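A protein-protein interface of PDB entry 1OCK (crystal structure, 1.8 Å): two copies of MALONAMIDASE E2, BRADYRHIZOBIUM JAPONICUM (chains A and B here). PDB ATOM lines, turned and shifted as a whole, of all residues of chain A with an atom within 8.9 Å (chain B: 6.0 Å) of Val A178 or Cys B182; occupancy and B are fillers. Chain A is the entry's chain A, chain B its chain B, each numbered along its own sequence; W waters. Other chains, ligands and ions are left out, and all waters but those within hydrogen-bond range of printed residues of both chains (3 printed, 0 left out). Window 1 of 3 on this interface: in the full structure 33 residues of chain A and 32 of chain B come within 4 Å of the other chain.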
ATOM      1  N   ILE A  64     -27.990  19.704  -5.511  1.00  0.00           N
ATOM      2  CA  ILE A  64     -28.322  18.356  -5.043  1.00  0.00           C
ATOM      3  C   ILE A  64     -27.197  17.481  -5.617  1.00  0.00           C
ATOM      4  O   ILE A  64     -27.165  16.263  -5.423  1.00  0.00           O
ATOM      5  CB  ILE A  64     -29.688  17.808  -5.554  1.00  0.00           C
ATOM      6  CG1 ILE A  64     -29.817  17.983  -7.067  1.00  0.00           C
ATOM      7  CG2 ILE A  64     -30.826  18.471  -4.791  1.00  0.00           C
ATOM      8  CD1 ILE A  64     -30.858  17.038  -7.697  1.00  0.00           C
ATOM      9  N   ILE A  65     -26.265  18.134  -6.309  1.00  0.00           N
ATOM     10  CA  ILE A  65     -25.121  17.464  -6.925  1.00  0.00           C
ATOM     11  C   ILE A  65     -23.862  17.706  -6.080  1.00  0.00           C
ATOM     12  O   ILE A  65     -23.473  18.850  -5.835  1.00  0.00           O
ATOM     13  CB  ILE A  65     -24.893  17.988  -8.366  1.00  0.00           C
ATOM     14  CG1 ILE A  65     -26.118  17.666  -9.230  1.00  0.00           C
ATOM     15  CG2 ILE A  65     -23.623  17.377  -8.950  1.00  0.00           C
ATOM     16  CD1 ILE A  65     -26.058  18.233 -10.635  1.00  0.00           C
ATOM     17  N   ASP A  66     -23.234  16.617  -5.644  1.00  0.00           N
ATOM     18  CA  ASP A  66     -22.042  16.674  -4.796  1.00  0.00           C
ATOM     19  C   ASP A  66     -20.825  17.427  -5.312  1.00  0.00           C
ATOM     20  O   ASP A  66     -20.410  17.267  -6.464  1.00  0.00           O
ATOM     21  CB  ASP A  66     -21.564  15.260  -4.438  1.00  0.00           C
ATOM     22  CG  ASP A  66     -22.486  14.545  -3.473  1.00  0.00           C
ATOM     23  OD1 ASP A  66     -23.439  15.167  -2.962  1.00  0.00           O
ATOM     24  OD2 ASP A  66     -22.238  13.347  -3.224  1.00  0.00           O
ATOM     25  N   THR A  67     -20.257  18.239  -4.424  1.00  0.00           N
ATOM     26  CA  THR A  67     -19.034  18.988  -4.680  1.00  0.00           C
ATOM     27  C   THR A  67     -18.204  18.783  -3.420  1.00  0.00           C
ATOM     28  O   THR A  67     -18.744  18.770  -2.314  1.00  0.00           O
ATOM     29  CB  THR A  67     -19.278  20.502  -4.900  1.00  0.00           C
ATOM     30  OG1 THR A  67     -20.189  21.003  -3.914  1.00  0.00           O
ATOM     31  CG2 THR A  67     -19.827  20.748  -6.290  1.00  0.00           C
ATOM     32  N   SER A  86     -16.486  13.839  -1.790  1.00  0.00           N
ATOM     33  CA  SER A  86     -16.073  13.876  -3.184  1.00  0.00           C
ATOM     34  C   SER A  86     -16.945  14.676  -4.138  1.00  0.00           C
ATOM     35  O   SER A  86     -18.082  15.025  -3.829  1.00  0.00           O
ATOM     36  CB  SER A  86     -15.993  12.448  -3.707  1.00  0.00           C
ATOM     37  OG  SER A  86     -17.276  11.847  -3.640  1.00  0.00           O
ATOM     38  N   ASP A  87     -16.379  14.959  -5.309  1.00  0.00           N
ATOM     39  CA  ASP A  87     -17.089  15.654  -6.373  1.00  0.00           C
ATOM     40  C   ASP A  87     -17.840  14.560  -7.115  1.00  0.00           C
ATOM     41  O   ASP A  87     -17.300  13.472  -7.337  1.00  0.00           O
ATOM     42  CB  ASP A  87     -16.113  16.315  -7.350  1.00  0.00           C
ATOM     43  CG  ASP A  87     -15.552  17.614  -6.826  1.00  0.00           C
ATOM     44  OD1 ASP A  87     -16.354  18.471  -6.406  1.00  0.00           O
ATOM     45  OD2 ASP A  87     -14.316  17.783  -6.850  1.00  0.00           O
ATOM     46  N   ALA A  88     -19.080  14.835  -7.499  1.00  0.00           N
ATOM     47  CA  ALA A  88     -19.859  13.840  -8.221  1.00  0.00           C
ATOM     48  C   ALA A  88     -19.222  13.579  -9.583  1.00  0.00           C
ATOM     49  O   ALA A  88     -18.589  14.459 -10.161  1.00  0.00           O
ATOM     50  CB  ALA A  88     -21.297  14.328  -8.400  1.00  0.00           C
ATOM     51  N   PRO A  89     -19.362  12.352 -10.101  1.00  0.00           N
ATOM     52  CA  PRO A  89     -18.787  12.026 -11.405  1.00  0.00           C
ATOM     53  C   PRO A  89     -19.096  13.058 -12.494  1.00  0.00           C
ATOM     54  O   PRO A  89     -18.211  13.403 -13.278  1.00  0.00           O
ATOM     55  CB  PRO A  89     -19.387  10.656 -11.699  1.00  0.00           C
ATOM     56  CG  PRO A  89     -19.363  10.023 -10.354  1.00  0.00           C
ATOM     57  CD  PRO A  89     -19.883  11.139  -9.446  1.00  0.00           C
ATOM     58  N   VAL A  90     -20.330  13.564 -12.552  1.00  0.00           N
ATOM     59  CA  VAL A  90     -20.641  14.551 -13.585  1.00  0.00           C
ATOM     60  C   VAL A  90     -19.865  15.843 -13.358  1.00  0.00           C
ATOM     61  O   VAL A  90     -19.549  16.554 -14.309  1.00  0.00           O
ATOM     62  CB  VAL A  90     -22.160  14.872 -13.678  1.00  0.00           C
ATOM     63  CG1 VAL A  90     -22.913  13.650 -14.170  1.00  0.00           C
ATOM     64  CG2 VAL A  90     -22.691  15.335 -12.332  1.00  0.00           C
ATOM     65  N   VAL A  91     -19.564  16.155 -12.100  1.00  0.00           N
ATOM     66  CA  VAL A  91     -18.786  17.354 -11.804  1.00  0.00           C
ATOM     67  C   VAL A  91     -17.351  17.125 -12.273  1.00  0.00           C
ATOM     68  O   VAL A  91     -16.717  18.023 -12.827  1.00  0.00           O
ATOM     69  CB  VAL A  91     -18.786  17.674 -10.297  1.00  0.00           C
ATOM     70  CG1 VAL A  91     -17.756  18.765  -9.988  1.00  0.00           C
ATOM     71  CG2 VAL A  91     -20.176  18.136  -9.877  1.00  0.00           C
ATOM     72  N   MET A  92     -16.843  15.914 -12.055  1.00  0.00           N
ATOM     73  CA  MET A  92     -15.488  15.578 -12.475  1.00  0.00           C
ATOM     74  C   MET A  92     -15.351  15.590 -13.998  1.00  0.00           C
ATOM     75  O   MET A  92     -14.278  15.884 -14.522  1.00  0.00           O
ATOM     76  CB  MET A  92     -15.079  14.204 -11.932  1.00  0.00           C
ATOM     77  CG  MET A  92     -14.784  14.183 -10.437  1.00  0.00           C
ATOM     78  SD  MET A  92     -13.526  15.387  -9.941  1.00  0.00           S
ATOM     79  CE  MET A  92     -12.070  14.748 -10.855  1.00  0.00           C
ATOM     80  N   ARG A 173     -29.999   7.782 -18.135  1.00  0.00           N
ATOM     81  CA  ARG A 173     -28.805   7.057 -17.714  1.00  0.00           C
ATOM     82  C   ARG A 173     -27.527   7.237 -18.531  1.00  0.00           C
ATOM     83  O   ARG A 173     -26.550   6.522 -18.299  1.00  0.00           O
ATOM     84  CB  ARG A 173     -29.117   5.561 -17.575  1.00  0.00           C
ATOM     85  CG  ARG A 173     -30.030   5.245 -16.398  1.00  0.00           C
ATOM     86  CD  ARG A 173     -30.188   3.742 -16.170  1.00  0.00           C
ATOM     87  NE  ARG A 173     -28.900   3.087 -15.955  1.00  0.00           N
ATOM     88  CZ  ARG A 173     -28.672   2.163 -15.026  1.00  0.00           C
ATOM     89  NH1 ARG A 173     -29.648   1.779 -14.214  1.00  0.00           N
ATOM     90  NH2 ARG A 173     -27.467   1.620 -14.908  1.00  0.00           N
ATOM     91  N   LEU A 175     -25.661  10.097 -18.643  1.00  0.00           N
ATOM     92  CA  LEU A 175     -24.783  10.764 -17.689  1.00  0.00           C
ATOM     93  C   LEU A 175     -25.069  10.101 -16.340  1.00  0.00           C
ATOM     94  O   LEU A 175     -26.224   9.879 -15.988  1.00  0.00           O
ATOM     95  CB  LEU A 175     -25.103  12.258 -17.625  1.00  0.00           C
ATOM     96  CG  LEU A 175     -24.852  13.070 -18.899  1.00  0.00           C
ATOM     97  CD1 LEU A 175     -25.278  14.513 -18.675  1.00  0.00           C
ATOM     98  CD2 LEU A 175     -23.374  13.003 -19.270  1.00  0.00           C
ATOM     99  N   PRO A 176     -24.022   9.767 -15.569  1.00  0.00           N
ATOM    100  CA  PRO A 176     -24.264   9.124 -14.274  1.00  0.00           C
ATOM    101  C   PRO A 176     -24.936  10.009 -13.229  1.00  0.00           C
ATOM    102  O   PRO A 176     -24.728  11.220 -13.199  1.00  0.00           O
ATOM    103  CB  PRO A 176     -22.869   8.681 -13.844  1.00  0.00           C
ATOM    104  CG  PRO A 176     -21.990   9.751 -14.432  1.00  0.00           C
ATOM    105  CD  PRO A 176     -22.579   9.942 -15.814  1.00  0.00           C
ATOM    106  N   THR A 177     -25.747   9.391 -12.376  1.00  0.00           N
ATOM    107  CA  THR A 177     -26.425  10.120 -11.311  1.00  0.00           C
ATOM    108  C   THR A 177     -25.746   9.869  -9.962  1.00  0.00           C
ATOM    109  O   THR A 177     -26.280  10.208  -8.899  1.00  0.00           O
ATOM    110  CB  THR A 177     -27.920   9.750 -11.248  1.00  0.00           C
ATOM    111  OG1 THR A 177     -28.081   8.332 -11.391  1.00  0.00           O
ATOM    112  CG2 THR A 177     -28.672  10.463 -12.369  1.00  0.00           C
ATOM    113  N   VAL A 178     -24.552   9.279 -10.015  1.00  0.00           N
ATOM    114  CA  VAL A 178     -23.768   9.032  -8.810  1.00  0.00           C
ATOM    115  C   VAL A 178     -23.473  10.417  -8.229  1.00  0.00           C
ATOM    116  O   VAL A 178     -23.138  11.340  -8.968  1.00  0.00           O
ATOM    117  CB  VAL A 178     -22.424   8.342  -9.147  1.00  0.00           C
ATOM    118  CG1 VAL A 178     -21.581   8.165  -7.890  1.00  0.00           C
ATOM    119  CG2 VAL A 178     -22.689   6.999  -9.806  1.00  0.00           C
ATOM    120  N   GLY A 179     -23.602  10.561  -6.916  1.00  0.00           N
ATOM    121  CA  GLY A 179     -23.342  11.849  -6.294  1.00  0.00           C
ATOM    122  C   GLY A 179     -24.442  12.867  -6.539  1.00  0.00           C
ATOM    123  O   GLY A 179     -24.245  14.066  -6.326  1.00  0.00           O
ATOM    124  N   VAL A 180     -25.600  12.396  -6.989  1.00  0.00           N
ATOM    125  CA  VAL A 180     -26.742  13.271  -7.253  1.00  0.00           C
ATOM    126  C   VAL A 180     -27.912  12.800  -6.385  1.00  0.00           C
ATOM    127  O   VAL A 180     -28.415  11.691  -6.566  1.00  0.00           O
ATOM    128  CB  VAL A 180     -27.163  13.210  -8.741  1.00  0.00           C
ATOM    129  CG1 VAL A 180     -28.369  14.114  -8.983  1.00  0.00           C
ATOM    130  CG2 VAL A 180     -25.990  13.627  -9.641  1.00  0.00           C
ATOM    131  N   LYS A 181     -28.342  13.639  -5.442  1.00  0.00           N
ATOM    132  CA  LYS A 181     -29.435  13.277  -4.541  1.00  0.00           C
ATOM    133  C   LYS A 181     -30.596  12.682  -5.327  1.00  0.00           C
ATOM    134  O   LYS A 181     -31.123  13.303  -6.253  1.00  0.00           O
ATOM    135  CB  LYS A 181     -29.900  14.503  -3.746  1.00  0.00           C
ATOM    136  CG  LYS A 181     -30.891  14.185  -2.629  1.00  0.00           C
ATOM    137  CD  LYS A 181     -30.277  13.281  -1.566  1.00  0.00           C
ATOM    138  CE  LYS A 181     -31.269  13.033  -0.437  1.00  0.00           C
ATOM    139  NZ  LYS A 181     -30.838  11.944   0.470  1.00  0.00           N
ATOM    140  N   CYS A 182     -30.995  11.473  -4.948  1.00  0.00           N
ATOM    141  CA  CYS A 182     -32.063  10.764  -5.636  1.00  0.00           C
ATOM    142  C   CYS A 182     -33.473  11.064  -5.148  1.00  0.00           C
ATOM    143  O   CYS A 182     -33.717  11.195  -3.947  1.00  0.00           O
ATOM    144  CB  CYS A 182     -31.820   9.252  -5.539  1.00  0.00           C
ATOM    145  SG  CYS A 182     -33.104   8.213  -6.311  1.00  0.00           S
ATOM    146  N   ASP A 188     -34.737  10.044 -12.366  1.00  0.00           N
ATOM    147  CA  ASP A 188     -33.669  11.045 -12.248  1.00  0.00           C
ATOM    148  C   ASP A 188     -32.696  11.017 -13.429  1.00  0.00           C
ATOM    149  O   ASP A 188     -32.102   9.982 -13.731  1.00  0.00           O
ATOM    150  CB  ASP A 188     -32.864  10.855 -10.959  1.00  0.00           C
ATOM    151  CG  ASP A 188     -33.679  11.114  -9.697  1.00  0.00           C
ATOM    152  OD1 ASP A 188     -34.842  11.573  -9.781  1.00  0.00           O
ATOM    153  OD2 ASP A 188     -33.136  10.852  -8.606  1.00  0.00           O
ATOM    154  N   VAL A 190     -29.635  13.707 -15.298  1.00  0.00           N
ATOM    155  CA  VAL A 190     -28.867  14.950 -15.255  1.00  0.00           C
ATOM    156  C   VAL A 190     -29.045  15.706 -16.573  1.00  0.00           C
ATOM    157  O   VAL A 190     -29.059  15.099 -17.640  1.00  0.00           O
ATOM    158  CB  VAL A 190     -27.363  14.659 -15.042  1.00  0.00           C
ATOM    159  CG1 VAL A 190     -26.558  15.950 -15.101  1.00  0.00           C
ATOM    160  CG2 VAL A 190     -27.160  13.970 -13.706  1.00  0.00           C
ATOM    161  N   PHE B 110     -13.130   0.154  -2.196  1.00  0.00           N
ATOM    162  CA  PHE B 110     -14.051   0.484  -3.282  1.00  0.00           C
ATOM    163  C   PHE B 110     -14.604  -0.755  -3.977  1.00  0.00           C
ATOM    164  O   PHE B 110     -14.905  -0.735  -5.172  1.00  0.00           O
ATOM    165  CB  PHE B 110     -13.370   1.407  -4.296  1.00  0.00           C
ATOM    166  CG  PHE B 110     -12.852   2.680  -3.688  1.00  0.00           C
ATOM    167  CD1 PHE B 110     -11.489   2.871  -3.496  1.00  0.00           C
ATOM    168  CD2 PHE B 110     -13.734   3.671  -3.266  1.00  0.00           C
ATOM    169  CE1 PHE B 110     -11.009   4.027  -2.891  1.00  0.00           C
ATOM    170  CE2 PHE B 110     -13.262   4.831  -2.660  1.00  0.00           C
ATOM    171  CZ  PHE B 110     -11.899   5.009  -2.471  1.00  0.00           C
ATOM    172  N   VAL B 180     -25.046   3.702  -2.149  1.00  0.00           N
ATOM    173  CA  VAL B 180     -24.127   2.570  -2.270  1.00  0.00           C
ATOM    174  C   VAL B 180     -22.983   3.023  -3.180  1.00  0.00           C
ATOM    175  O   VAL B 180     -23.205   3.318  -4.355  1.00  0.00           O
ATOM    176  CB  VAL B 180     -24.820   1.336  -2.899  1.00  0.00           C
ATOM    177  CG1 VAL B 180     -23.817   0.198  -3.039  1.00  0.00           C
ATOM    178  CG2 VAL B 180     -26.003   0.898  -2.037  1.00  0.00           C
ATOM    179  N   LYS B 181     -21.769   3.088  -2.630  1.00  0.00           N
ATOM    180  CA  LYS B 181     -20.600   3.532  -3.388  1.00  0.00           C
ATOM    181  C   LYS B 181     -20.563   2.841  -4.743  1.00  0.00           C
ATOM    182  O   LYS B 181     -20.498   1.620  -4.820  1.00  0.00           O
ATOM    183  CB  LYS B 181     -19.316   3.229  -2.611  1.00  0.00           C
ATOM    184  CG  LYS B 181     -18.057   3.820  -3.238  1.00  0.00           C
ATOM    185  CD  LYS B 181     -18.138   5.336  -3.309  1.00  0.00           C
ATOM    186  CE  LYS B 181     -16.864   5.933  -3.891  1.00  0.00           C
ATOM    187  NZ  LYS B 181     -17.073   7.351  -4.274  1.00  0.00           N
ATOM    188  N   CYS B 182     -20.588   3.636  -5.805  1.00  0.00           N
ATOM    189  CA  CYS B 182     -20.604   3.102  -7.158  1.00  0.00           C
ATOM    190  C   CYS B 182     -19.253   2.731  -7.754  1.00  0.00           C
ATOM    191  O   CYS B 182     -18.263   3.443  -7.589  1.00  0.00           O
ATOM    192  CB  CYS B 182     -21.305   4.103  -8.084  1.00  0.00           C
ATOM    193  SG  CYS B 182     -21.469   3.546  -9.800  1.00  0.00           S
ATOM    194  N   TYR B 183     -19.225   1.594  -8.441  1.00  0.00           N
ATOM    195  CA  TYR B 183     -18.024   1.147  -9.124  1.00  0.00           C
ATOM    196  C   TYR B 183     -18.404   1.198 -10.603  1.00  0.00           C
ATOM    197  O   TYR B 183     -17.738   1.844 -11.407  1.00  0.00           O
ATOM    198  CB  TYR B 183     -17.647  -0.275  -8.711  1.00  0.00           C
ATOM    199  CG  TYR B 183     -16.285  -0.680  -9.218  1.00  0.00           C
ATOM    200  CD1 TYR B 183     -16.136  -1.336 -10.439  1.00  0.00           C
ATOM    201  CD2 TYR B 183     -15.137  -0.379  -8.487  1.00  0.00           C
ATOM    202  CE1 TYR B 183     -14.875  -1.685 -10.917  1.00  0.00           C
ATOM    203  CE2 TYR B 183     -13.874  -0.717  -8.957  1.00  0.00           C
ATOM    204  CZ  TYR B 183     -13.751  -1.372 -10.169  1.00  0.00           C
ATOM    205  OH  TYR B 183     -12.502  -1.718 -10.620  1.00  0.00           O
ATOM    206  N   SER B 184     -19.503   0.534 -10.938  1.00  0.00           N
ATOM    207  CA  SER B 184     -20.030   0.517 -12.301  1.00  0.00           C
ATOM    208  C   SER B 184     -21.553   0.541 -12.189  1.00  0.00           C
ATOM    209  O   SER B 184     -22.160  -0.425 -11.741  1.00  0.00           O
ATOM    210  CB  SER B 184     -19.578  -0.746 -13.036  1.00  0.00           C
ATOM    211  OG  SER B 184     -20.215  -0.841 -14.299  1.00  0.00           O
ATOM    212  N   TRP B 185     -22.177   1.642 -12.596  1.00  0.00           N
ATOM    213  CA  TRP B 185     -23.627   1.744 -12.486  1.00  0.00           C
ATOM    214  C   TRP B 185     -24.382   0.786 -13.398  1.00  0.00           C
ATOM    215  O   TRP B 185     -25.543   0.462 -13.153  1.00  0.00           O
ATOM    216  CB  TRP B 185     -24.079   3.196 -12.714  1.00  0.00           C
ATOM    217  CG  TRP B 185     -23.691   3.801 -14.028  1.00  0.00           C
ATOM    218  CD1 TRP B 185     -24.395   3.740 -15.197  1.00  0.00           C
ATOM    219  CD2 TRP B 185     -22.520   4.583 -14.305  1.00  0.00           C
ATOM    220  NE1 TRP B 185     -23.740   4.437 -16.182  1.00  0.00           N
ATOM    221  CE2 TRP B 185     -22.586   4.964 -15.665  1.00  0.00           C
ATOM    222  CE3 TRP B 185     -21.422   4.998 -13.539  1.00  0.00           C
ATOM    223  CZ2 TRP B 185     -21.597   5.743 -16.275  1.00  0.00           C
ATOM    224  CZ3 TRP B 185     -20.437   5.773 -14.146  1.00  0.00           C
ATOM    225  CH2 TRP B 185     -20.533   6.137 -15.501  1.00  0.00           C
ATOM    226  N   ASP B 188     -23.447  -2.633 -10.690  1.00  0.00           N
ATOM    227  CA  ASP B 188     -23.673  -2.702  -9.242  1.00  0.00           C
ATOM    228  C   ASP B 188     -25.069  -3.183  -8.856  1.00  0.00           C
ATOM    229  O   ASP B 188     -26.075  -2.603  -9.268  1.00  0.00           O
ATOM    230  CB  ASP B 188     -23.424  -1.345  -8.559  1.00  0.00           C
ATOM    231  CG  ASP B 188     -21.991  -0.849  -8.715  1.00  0.00           C
ATOM    232  OD1 ASP B 188     -21.114  -1.617  -9.162  1.00  0.00           O
ATOM    233  OD2 ASP B 188     -21.742   0.327  -8.372  1.00  0.00           O
ATOM    234  N   ALA B 284     -16.894   6.677 -12.379  1.00  0.00           N
ATOM    235  CA  ALA B 284     -17.465   6.591 -11.031  1.00  0.00           C
ATOM    236  C   ALA B 284     -16.483   6.929  -9.909  1.00  0.00           C
ATOM    237  O   ALA B 284     -16.879   7.439  -8.858  1.00  0.00           O
ATOM    238  CB  ALA B 284     -18.055   5.198 -10.806  1.00  0.00           C
ATOM    239  N   LEU B 285     -15.206   6.637 -10.123  1.00  0.00           N
ATOM    240  CA  LEU B 285     -14.176   6.922  -9.129  1.00  0.00           C
ATOM    241  C   LEU B 285     -13.246   8.021  -9.641  1.00  0.00           C
ATOM    242  O   LEU B 285     -12.070   8.061  -9.289  1.00  0.00           O
ATOM    243  CB  LEU B 285     -13.362   5.658  -8.836  1.00  0.00           C
ATOM    244  CG  LEU B 285     -14.140   4.474  -8.258  1.00  0.00           C
ATOM    245  CD1 LEU B 285     -13.246   3.242  -8.220  1.00  0.00           C
ATOM    246  CD2 LEU B 285     -14.637   4.831  -6.857  1.00  0.00           C
HETATM  247  O   HOH W   1     -17.987   9.748  -5.088  1.00  0.00           O
HETATM  248  O   HOH W   2     -26.406   6.174 -15.303  1.00  0.00           O
HETATM  249  O   HOH W   3     -24.562   4.967 -18.894  1.00  0.00           O
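The backbone carbonyl oxygen (O) of Trp B185 is in hydrogen-bond range of the guanidinium group (NH2) of Arg A173, at 2.9 Å.
N of Ser B184 sits at hydrogen-bond distance from SG of Cys B182, at 3.8 Å. OD2 of Asp B188 sits close to SG of Cys B182, 3.5 Å away. The side-chain sulfur (SG) of Cys B182 sits at hydrogen-bond distance from the backbone NH (N) of Trp B185 (3.5 Å).
Among the printed residues, merely in contact across the chains: Val A178 with Cys B182 (3.6 Å), Pro A176 with Trp B185 (3.8 Å) and Pro A89 with Ala B284 (3.9 Å).
Of the printed residues of chain B, Pro A89 touches Ala B284. Of the printed residues of chain B, Arg A173 touches Trp B185. Of the printed residues of chain B, Pro A176 touches Trp B185. Val A178 touches just one residue of chain B: Cys B182. Cys B182 touches just one residue of chain A: Val A178. Of the printed residues of chain A, Ala B284 touches Pro A89. The nearest residue of chain B that does not touch Val A178 is Trp B185 (4.4 Å).
Of the 10 printed residues of chain B, 3 touch a printed residue of chain A. Hydrophobic or aromatic side chains of chain B that line the printed part of chain A: Trp B185. Of the 22 printed residues of chain A, 4 touch a printed residue of chain B. Among the printed residues, no Asp or Glu carboxylate lies within 4 Å of a Lys or Arg side-chain nitrogen of the other chain.
4 positions are printed for both chains.
Water W3 bridges the backbone carbonyl oxygen of Arg A173 (2.6 Å) and the indole nitrogen of Trp B185 (2.9 Å). Water W1 bridges OG of Ser A86 (2.6 Å) and NZ of Lys B181 (2.7 Å). Water W2 bridges the backbone carbonyl oxygen of Arg A173 (3.0 Å) and the indole nitrogen of Trp B185 (3.3 Å).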
